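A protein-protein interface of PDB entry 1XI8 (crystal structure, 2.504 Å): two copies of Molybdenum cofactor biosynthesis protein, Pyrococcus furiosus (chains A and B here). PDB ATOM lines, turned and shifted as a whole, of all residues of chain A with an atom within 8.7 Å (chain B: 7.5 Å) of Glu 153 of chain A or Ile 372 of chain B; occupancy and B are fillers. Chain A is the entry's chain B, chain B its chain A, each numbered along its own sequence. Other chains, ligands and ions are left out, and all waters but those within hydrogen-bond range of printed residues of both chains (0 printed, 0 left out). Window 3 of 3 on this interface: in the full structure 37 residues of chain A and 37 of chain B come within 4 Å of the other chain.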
ATOM      1  N   ASP A  56     -16.092  -3.530  39.178  1.00  0.00           N
ATOM      2  CA  ASP A  56     -15.702  -4.430  38.093  1.00  0.00           C
ATOM      3  C   ASP A  56     -16.620  -4.268  36.885  1.00  0.00           C
ATOM      4  O   ASP A  56     -17.781  -3.856  37.027  1.00  0.00           O
ATOM      5  CB  ASP A  56     -15.771  -5.895  38.536  1.00  0.00           C
ATOM      6  CG  ASP A  56     -14.645  -6.291  39.485  1.00  0.00           C
ATOM      7  OD1 ASP A  56     -13.480  -5.832  39.325  1.00  0.00           O
ATOM      8  OD2 ASP A  56     -14.930  -7.098  40.392  1.00  0.00           O
ATOM      9  N   LEU A  57     -16.101  -4.597  35.700  1.00  0.00           N
ATOM     10  CA  LEU A  57     -16.954  -4.774  34.524  1.00  0.00           C
ATOM     11  C   LEU A  57     -16.945  -6.242  34.128  1.00  0.00           C
ATOM     12  O   LEU A  57     -17.492  -7.075  34.870  1.00  0.00           O
ATOM     13  CB  LEU A  57     -16.505  -3.894  33.359  1.00  0.00           C
ATOM     14  CG  LEU A  57     -16.580  -2.385  33.600  1.00  0.00           C
ATOM     15  CD1 LEU A  57     -15.986  -1.690  32.406  1.00  0.00           C
ATOM     16  CD2 LEU A  57     -18.025  -1.948  33.835  1.00  0.00           C
ATOM     17  N   SER A 149     -17.314 -16.688  31.182  1.00  0.00           N
ATOM     18  CA  SER A 149     -16.816 -15.319  31.236  1.00  0.00           C
ATOM     19  C   SER A 149     -16.779 -14.849  32.686  1.00  0.00           C
ATOM     20  O   SER A 149     -17.612 -14.032  33.104  1.00  0.00           O
ATOM     21  CB  SER A 149     -17.704 -14.381  30.397  1.00  0.00           C
ATOM     22  OG  SER A 149     -17.166 -13.060  30.343  1.00  0.00           O
ATOM     23  N   PHE A 150     -15.831 -15.379  33.462  1.00  0.00           N
ATOM     24  CA  PHE A 150     -15.677 -14.913  34.837  1.00  0.00           C
ATOM     25  C   PHE A 150     -15.074 -13.520  34.679  1.00  0.00           C
ATOM     26  O   PHE A 150     -13.970 -13.347  34.114  1.00  0.00           O
ATOM     27  CB  PHE A 150     -14.893 -15.903  35.745  1.00  0.00           C
ATOM     28  CG  PHE A 150     -13.380 -15.829  35.622  1.00  0.00           C
ATOM     29  CD1 PHE A 150     -12.610 -15.289  36.671  1.00  0.00           C
ATOM     30  CD2 PHE A 150     -12.725 -16.316  34.480  1.00  0.00           C
ATOM     31  CE1 PHE A 150     -11.209 -15.226  36.580  1.00  0.00           C
ATOM     32  CE2 PHE A 150     -11.322 -16.261  34.376  1.00  0.00           C
ATOM     33  CZ  PHE A 150     -10.563 -15.711  35.425  1.00  0.00           C
ATOM     34  N   ALA A 151     -15.847 -12.543  35.165  1.00  0.00           N
ATOM     35  CA  ALA A 151     -15.716 -11.131  34.793  1.00  0.00           C
ATOM     36  C   ALA A 151     -14.803 -10.284  35.682  1.00  0.00           C
ATOM     37  O   ALA A 151     -14.384 -10.700  36.776  1.00  0.00           O
ATOM     38  CB  ALA A 151     -17.112 -10.485  34.679  1.00  0.00           C
ATOM     39  N   GLY A 152     -14.560  -9.064  35.195  1.00  0.00           N
ATOM     40  CA  GLY A 152     -13.408  -8.270  35.571  1.00  0.00           C
ATOM     41  C   GLY A 152     -12.465  -8.393  34.371  1.00  0.00           C
ATOM     42  O   GLY A 152     -11.259  -8.173  34.496  1.00  0.00           O
ATOM     43  N   GLU A 153     -13.002  -8.771  33.205  1.00  0.00           N
ATOM     44  CA  GLU A 153     -12.176  -8.923  31.993  1.00  0.00           C
ATOM     45  C   GLU A 153     -11.897  -7.544  31.411  1.00  0.00           C
ATOM     46  O   GLU A 153     -10.769  -7.208  31.043  1.00  0.00           O
ATOM     47  CB  GLU A 153     -12.890  -9.735  30.908  1.00  0.00           C
ATOM     48  CG  GLU A 153     -13.210 -11.205  31.195  1.00  0.00           C
ATOM     49  CD  GLU A 153     -14.218 -11.747  30.172  1.00  0.00           C
ATOM     50  OE1 GLU A 153     -15.295 -11.111  29.990  1.00  0.00           O
ATOM     51  OE2 GLU A 153     -13.929 -12.809  29.547  1.00  0.00           O
ATOM     52  N   ASP A 154     -12.964  -6.757  31.323  1.00  0.00           N
ATOM     53  CA  ASP A 154     -12.896  -5.412  30.800  1.00  0.00           C
ATOM     54  C   ASP A 154     -11.894  -4.602  31.623  1.00  0.00           C
ATOM     55  O   ASP A 154     -10.795  -4.345  31.155  1.00  0.00           O
ATOM     56  CB  ASP A 154     -14.298  -4.799  30.801  1.00  0.00           C
ATOM     57  CG  ASP A 154     -14.450  -3.675  29.790  1.00  0.00           C
ATOM     58  OD1 ASP A 154     -13.497  -2.865  29.643  1.00  0.00           O
ATOM     59  OD2 ASP A 154     -15.530  -3.598  29.152  1.00  0.00           O
ATOM     60  N   VAL A 155     -12.255  -4.214  32.845  1.00  0.00           N
ATOM     61  CA  VAL A 155     -11.301  -3.557  33.760  1.00  0.00           C
ATOM     62  C   VAL A 155     -11.655  -3.867  35.216  1.00  0.00           C
ATOM     63  O   VAL A 155     -12.838  -3.853  35.579  1.00  0.00           O
ATOM     64  CB  VAL A 155     -11.241  -2.023  33.563  1.00  0.00           C
ATOM     65  CG1 VAL A 155     -12.554  -1.376  33.967  1.00  0.00           C
ATOM     66  CG2 VAL A 155     -10.087  -1.421  34.366  1.00  0.00           C
ATOM     67  N   LYS A 156     -10.639  -4.151  36.037  1.00  0.00           N
ATOM     68  CA  LYS A 156     -10.858  -4.509  37.441  1.00  0.00           C
ATOM     69  C   LYS A 156     -10.808  -3.296  38.372  1.00  0.00           C
ATOM     70  O   LYS A 156     -10.050  -2.336  38.135  1.00  0.00           O
ATOM     71  CB  LYS A 156      -9.840  -5.556  37.901  1.00  0.00           C
ATOM     72  N   LYS A 157     -11.620  -3.352  39.429  1.00  0.00           N
ATOM     73  CA  LYS A 157     -11.654  -2.306  40.440  1.00  0.00           C
ATOM     74  C   LYS A 157     -10.230  -2.010  40.899  1.00  0.00           C
ATOM     75  O   LYS A 157      -9.469  -2.931  41.227  1.00  0.00           O
ATOM     76  CB  LYS A 157     -12.537  -2.729  41.618  1.00  0.00           C
ATOM     77  N   ASP A 159      -7.838  -0.799  38.954  1.00  0.00           N
ATOM     78  CA  ASP A 159      -6.967  -0.666  37.779  1.00  0.00           C
ATOM     79  C   ASP A 159      -7.183   0.676  37.120  1.00  0.00           C
ATOM     80  O   ASP A 159      -8.260   1.272  37.255  1.00  0.00           O
ATOM     81  CB  ASP A 159      -7.235  -1.777  36.781  1.00  0.00           C
ATOM     82  CG  ASP A 159      -6.523  -3.049  37.142  1.00  0.00           C
ATOM     83  OD1 ASP A 159      -5.432  -2.954  37.747  1.00  0.00           O
ATOM     84  OD2 ASP A 159      -7.039  -4.144  36.821  1.00  0.00           O
ATOM     85  N   GLN A 171     -14.486   5.643  21.833  1.00  0.00           N
ATOM     86  CA  GLN A 171     -14.494   4.450  22.686  1.00  0.00           C
ATOM     87  C   GLN A 171     -14.063   4.791  24.120  1.00  0.00           C
ATOM     88  O   GLN A 171     -14.405   4.084  25.061  1.00  0.00           O
ATOM     89  CB  GLN A 171     -13.643   3.315  22.097  1.00  0.00           C
ATOM     90  CG  GLN A 171     -12.158   3.633  21.877  1.00  0.00           C
ATOM     91  CD  GLN A 171     -11.854   4.214  20.502  1.00  0.00           C
ATOM     92  OE1 GLN A 171     -12.494   5.164  20.057  1.00  0.00           O
ATOM     93  NE2 GLN A 171     -10.871   3.644  19.828  1.00  0.00           N
ATOM     94  N   LEU A 175     -16.204   4.000  27.465  1.00  0.00           N
ATOM     95  CA  LEU A 175     -15.713   3.364  28.685  1.00  0.00           C
ATOM     96  C   LEU A 175     -16.088   4.192  29.904  1.00  0.00           C
ATOM     97  O   LEU A 175     -16.609   3.664  30.883  1.00  0.00           O
ATOM     98  CB  LEU A 175     -14.198   3.135  28.632  1.00  0.00           C
ATOM     99  CG  LEU A 175     -13.615   2.419  29.863  1.00  0.00           C
ATOM    100  CD1 LEU A 175     -14.421   1.162  30.258  1.00  0.00           C
ATOM    101  CD2 LEU A 175     -12.146   2.072  29.646  1.00  0.00           C
ATOM    102  N   TYR B 306     -23.578  -5.097  21.316  1.00  0.00           N
ATOM    103  CA  TYR B 306     -22.297  -5.204  21.999  1.00  0.00           C
ATOM    104  C   TYR B 306     -21.327  -4.155  21.476  1.00  0.00           C
ATOM    105  O   TYR B 306     -21.058  -4.098  20.280  1.00  0.00           O
ATOM    106  CB  TYR B 306     -21.696  -6.610  21.869  1.00  0.00           C
ATOM    107  CG  TYR B 306     -22.678  -7.734  22.159  1.00  0.00           C
ATOM    108  CD1 TYR B 306     -23.081  -8.618  21.149  1.00  0.00           C
ATOM    109  CD2 TYR B 306     -23.209  -7.911  23.436  1.00  0.00           C
ATOM    110  CE1 TYR B 306     -23.980  -9.648  21.408  1.00  0.00           C
ATOM    111  CE2 TYR B 306     -24.108  -8.933  23.710  1.00  0.00           C
ATOM    112  CZ  TYR B 306     -24.493  -9.797  22.696  1.00  0.00           C
ATOM    113  OH  TYR B 306     -25.393 -10.812  22.973  1.00  0.00           O
ATOM    114  N   PRO B 307     -20.803  -3.314  22.385  1.00  0.00           N
ATOM    115  CA  PRO B 307     -19.860  -2.238  22.101  1.00  0.00           C
ATOM    116  C   PRO B 307     -18.811  -2.550  21.026  1.00  0.00           C
ATOM    117  O   PRO B 307     -18.629  -1.737  20.124  1.00  0.00           O
ATOM    118  CB  PRO B 307     -19.181  -2.024  23.447  1.00  0.00           C
ATOM    119  CG  PRO B 307     -20.216  -2.348  24.425  1.00  0.00           C
ATOM    120  CD  PRO B 307     -21.143  -3.360  23.816  1.00  0.00           C
ATOM    121  N   VAL B 308     -18.131  -3.695  21.117  1.00  0.00           N
ATOM    122  CA  VAL B 308     -17.059  -3.998  20.162  1.00  0.00           C
ATOM    123  C   VAL B 308     -17.630  -4.392  18.791  1.00  0.00           C
ATOM    124  O   VAL B 308     -17.042  -4.085  17.767  1.00  0.00           O
ATOM    125  CB  VAL B 308     -16.046  -5.052  20.692  1.00  0.00           C
ATOM    126  CG1 VAL B 308     -16.611  -6.393  20.571  1.00  0.00           C
ATOM    127  CG2 VAL B 308     -14.771  -5.030  19.880  1.00  0.00           C
ATOM    128  N   ALA B 309     -18.779  -5.056  18.785  1.00  0.00           N
ATOM    129  CA  ALA B 309     -19.471  -5.375  17.542  1.00  0.00           C
ATOM    130  C   ALA B 309     -19.991  -4.107  16.865  1.00  0.00           C
ATOM    131  O   ALA B 309     -19.935  -3.979  15.653  1.00  0.00           O
ATOM    132  CB  ALA B 309     -20.618  -6.353  17.799  1.00  0.00           C
ATOM    133  N   LYS B 366      -5.371  -8.719  22.992  1.00  0.00           N
ATOM    134  CA  LYS B 366      -6.032  -9.956  23.401  1.00  0.00           C
ATOM    135  C   LYS B 366      -7.296  -9.624  24.186  1.00  0.00           C
ATOM    136  O   LYS B 366      -7.212  -9.058  25.269  1.00  0.00           O
ATOM    137  CB  LYS B 366      -5.081 -10.798  24.262  1.00  0.00           C
ATOM    138  N   LYS B 367      -8.464  -9.956  23.642  1.00  0.00           N
ATOM    139  CA  LYS B 367      -9.736  -9.771  24.366  1.00  0.00           C
ATOM    140  C   LYS B 367     -10.928  -9.817  23.418  1.00  0.00           C
ATOM    141  O   LYS B 367     -11.506 -10.882  23.193  1.00  0.00           O
ATOM    142  CB  LYS B 367      -9.750  -8.468  25.187  1.00  0.00           C
ATOM    143  N   GLY B 369     -20.031  -9.875  18.339  1.00  0.00           N
ATOM    144  CA  GLY B 369     -19.345  -8.852  19.146  1.00  0.00           C
ATOM    145  C   GLY B 369     -18.704  -9.334  20.442  1.00  0.00           C
ATOM    146  O   GLY B 369     -18.457 -10.531  20.617  1.00  0.00           O
ATOM    147  N   SER B 370     -18.440  -8.387  21.344  1.00  0.00           N
ATOM    148  CA  SER B 370     -17.839  -8.643  22.658  1.00  0.00           C
ATOM    149  C   SER B 370     -18.134  -7.440  23.571  1.00  0.00           C
ATOM    150  O   SER B 370     -17.917  -6.287  23.188  1.00  0.00           O
ATOM    151  CB  SER B 370     -16.321  -8.896  22.530  1.00  0.00           C
ATOM    152  OG  SER B 370     -15.609  -8.635  23.749  1.00  0.00           O
ATOM    153  N   GLY B 371     -18.642  -7.700  24.775  1.00  0.00           N
ATOM    154  CA  GLY B 371     -19.008  -6.613  25.691  1.00  0.00           C
ATOM    155  C   GLY B 371     -17.830  -5.832  26.263  1.00  0.00           C
ATOM    156  O   GLY B 371     -18.027  -4.911  27.073  1.00  0.00           O
ATOM    157  N   ILE B 372     -16.619  -6.174  25.817  1.00  0.00           N
ATOM    158  CA  ILE B 372     -15.381  -5.684  26.422  1.00  0.00           C
ATOM    159  C   ILE B 372     -14.735  -4.486  25.715  1.00  0.00           C
ATOM    160  O   ILE B 372     -13.739  -4.639  24.991  1.00  0.00           O
ATOM    161  CB  ILE B 372     -14.353  -6.837  26.505  1.00  0.00           C
ATOM    162  CG1 ILE B 372     -15.027  -8.083  27.100  1.00  0.00           C
ATOM    163  CG2 ILE B 372     -13.098  -6.410  27.294  1.00  0.00           C
ATOM    164  CD1 ILE B 372     -14.308  -9.378  26.806  1.00  0.00           C
ATOM    165  N   ILE B 373     -15.273  -3.291  25.958  1.00  0.00           N
ATOM    166  CA  ILE B 373     -14.784  -2.080  25.303  1.00  0.00           C
ATOM    167  C   ILE B 373     -13.330  -1.701  25.625  1.00  0.00           C
ATOM    168  O   ILE B 373     -12.806  -0.731  25.065  1.00  0.00           O
ATOM    169  CB  ILE B 373     -15.682  -0.861  25.625  1.00  0.00           C
ATOM    170  CG1 ILE B 373     -15.501  -0.418  27.059  1.00  0.00           C
ATOM    171  CG2 ILE B 373     -17.139  -1.201  25.481  1.00  0.00           C
ATOM    172  CD1 ILE B 373     -16.616   0.512  27.496  1.00  0.00           C
ATOM    173  N   SER B 374     -12.664  -2.428  26.518  1.00  0.00           N
ATOM    174  CA  SER B 374     -11.267  -2.064  26.822  1.00  0.00           C
ATOM    175  C   SER B 374     -10.329  -2.399  25.651  1.00  0.00           C
ATOM    176  O   SER B 374      -9.285  -1.768  25.495  1.00  0.00           O
ATOM    177  CB  SER B 374     -10.766  -2.682  28.138  1.00  0.00           C
ATOM    178  OG  SER B 374     -10.362  -4.024  27.941  1.00  0.00           O
ATOM    179  N   SER B 375     -10.700  -3.382  24.832  1.00  0.00           N
ATOM    180  CA  SER B 375      -9.903  -3.694  23.641  1.00  0.00           C
ATOM    181  C   SER B 375     -10.019  -2.570  22.617  1.00  0.00           C
ATOM    182  O   SER B 375      -9.092  -2.336  21.846  1.00  0.00           O
ATOM    183  CB  SER B 375     -10.277  -5.044  23.012  1.00  0.00           C
ATOM    184  OG  SER B 375     -11.641  -5.088  22.653  1.00  0.00           O
ATOM    185  N   LEU B 376     -11.147  -1.868  22.625  1.00  0.00           N
ATOM    186  CA  LEU B 376     -11.318  -0.722  21.748  1.00  0.00           C
ATOM    187  C   LEU B 376     -10.405   0.435  22.167  1.00  0.00           C
ATOM    188  O   LEU B 376      -9.816   1.115  21.314  1.00  0.00           O
ATOM    189  CB  LEU B 376     -12.784  -0.272  21.712  1.00  0.00           C
ATOM    190  CG  LEU B 376     -13.816  -1.292  21.208  1.00  0.00           C
ATOM    191  CD1 LEU B 376     -15.180  -0.652  21.063  1.00  0.00           C
ATOM    192  CD2 LEU B 376     -13.383  -1.918  19.890  1.00  0.00           C
ATOM    193  N   VAL B 377     -10.274   0.648  23.474  1.00  0.00           N
ATOM    194  CA  VAL B 377      -9.511   1.790  23.967  1.00  0.00           C
ATOM    195  C   VAL B 377      -8.018   1.522  23.973  1.00  0.00           C
ATOM    196  O   VAL B 377      -7.215   2.447  23.924  1.00  0.00           O
ATOM    197  CB  VAL B 377      -9.945   2.240  25.393  1.00  0.00           C
ATOM    198  CG1 VAL B 377     -11.454   2.318  25.508  1.00  0.00           C
ATOM    199  CG2 VAL B 377      -9.378   1.320  26.429  1.00  0.00           C
ATOM    200  N   GLN B 378      -7.634   0.256  24.037  1.00  0.00           N
ATOM    201  CA  GLN B 378      -6.210  -0.074  24.034  1.00  0.00           C
ATOM    202  C   GLN B 378      -5.683  -0.244  22.619  1.00  0.00           C
ATOM    203  O   GLN B 378      -4.531  -0.620  22.426  1.00  0.00           O
ATOM    204  CB  GLN B 378      -5.932  -1.323  24.863  1.00  0.00           C
ATOM    205  CG  GLN B 378      -6.111  -1.106  26.343  1.00  0.00           C
ATOM    206  CD  GLN B 378      -5.895  -2.385  27.134  1.00  0.00           C
ATOM    207  OE1 GLN B 378      -5.583  -3.441  26.562  1.00  0.00           O
ATOM    208  NE2 GLN B 378      -6.060  -2.303  28.461  1.00  0.00           N
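No position is printed for both chains. Of the 8 pairs that touch across the chains among the printed residues, none has its exchanged pair printed and touching as well.
Printed residues of chain A that touch a printed residue of chain B: Glu 153, Asp 154, Gln 171 and Leu 175. Hydrophobic or aromatic side chains of chain A within 4 Å of the printed part of chain B: Leu 175. Along chain A the printed residues that touch a printed residue of chain B span positions 153 to 175. Hydrophobic or aromatic side chains of chain B that line the printed part of chain A: Ile 372, Ile 373, Leu 376 and Val 377. Among the printed residues, no Asp or Glu carboxylate lies within 4 Å of a Lys or Arg side-chain nitrogen of the other chain.
Of chain B, only Ile 372 comes within 4 Å of Glu 153 of chain A. Ile 372 of chain B touches just these residues of chain A: Glu 153 and Asp 154. No residue of chain B comes within 4 Å of Gly 152 of chain A. Gly 371 of chain B touches one residue of chain A. Of the printed residues of chain A, Val 377 of chain B touches Gln 171 (3.5 Å). Of the printed residues of chain B, Gln 171 of chain A touches Leu 376 and Val 377. Of the printed residues of chain A, Ser 374 of chain B touches Asp 154. Printed residues of chain A within 4 Å of Ile 373 of chain B: Asp 154 (3.2 Å) and Leu 175 (3.2 Å). Of the printed residues of chain A, Leu 376 of chain B touches Gln 171. Lys 367 of chain B touches none of the printed residues of chain A. The nearest printed residue of chain A that does not touch Leu 376 of chain B is Asp 154 of chain A (7.5 Å).
The backbone NH of Ile 372 of chain B sits close to the side-chain hydroxyl of Ser 370 of chain B. The backbone carbonyl oxygen (O) of Ile 372 of chain B is in hydrogen-bond range of the side-chain hydroxyl (OG) of Ser 375 of chain B (3.2 Å). The side-chain carboxylate (OE1) of Glu 153 of chain A is in hydrogen-bond range of the side-chain hydroxyl (OG) of Ser 149 of chain A (2.7 Å).
Among the printed residues, pairs that only touch across the chains: Leu 175 of chain A with Ile 373 of chain B (3.2 Å), Asp 154 of chain A with Ile 372 of chain B (3.4 Å), Gln 171 of chain A with Val 377 of chain B (3.5 Å), Asp 154 of chain A with Gly 371 of chain B (3.5 Å) and Glu 153 of chain A with Ile 372 of chain B (3.8 Å).
N of Ile 373 of chain B sits at hydrogen-bond distance from OD2 of Asp 154 of chain A (3.2 Å). The backbone carbonyl oxygen (O) of Asp 154 of chain A sits at hydrogen-bond distance from the side-chain hydroxyl (OG) of Ser 374 of chain B, at 3.3 Å. The side-chain amide nitrogen (NE2) of Gln 171 of chain A lies within hydrogen-bond range of the backbone carbonyl oxygen (O) of Leu 376 of chain B.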
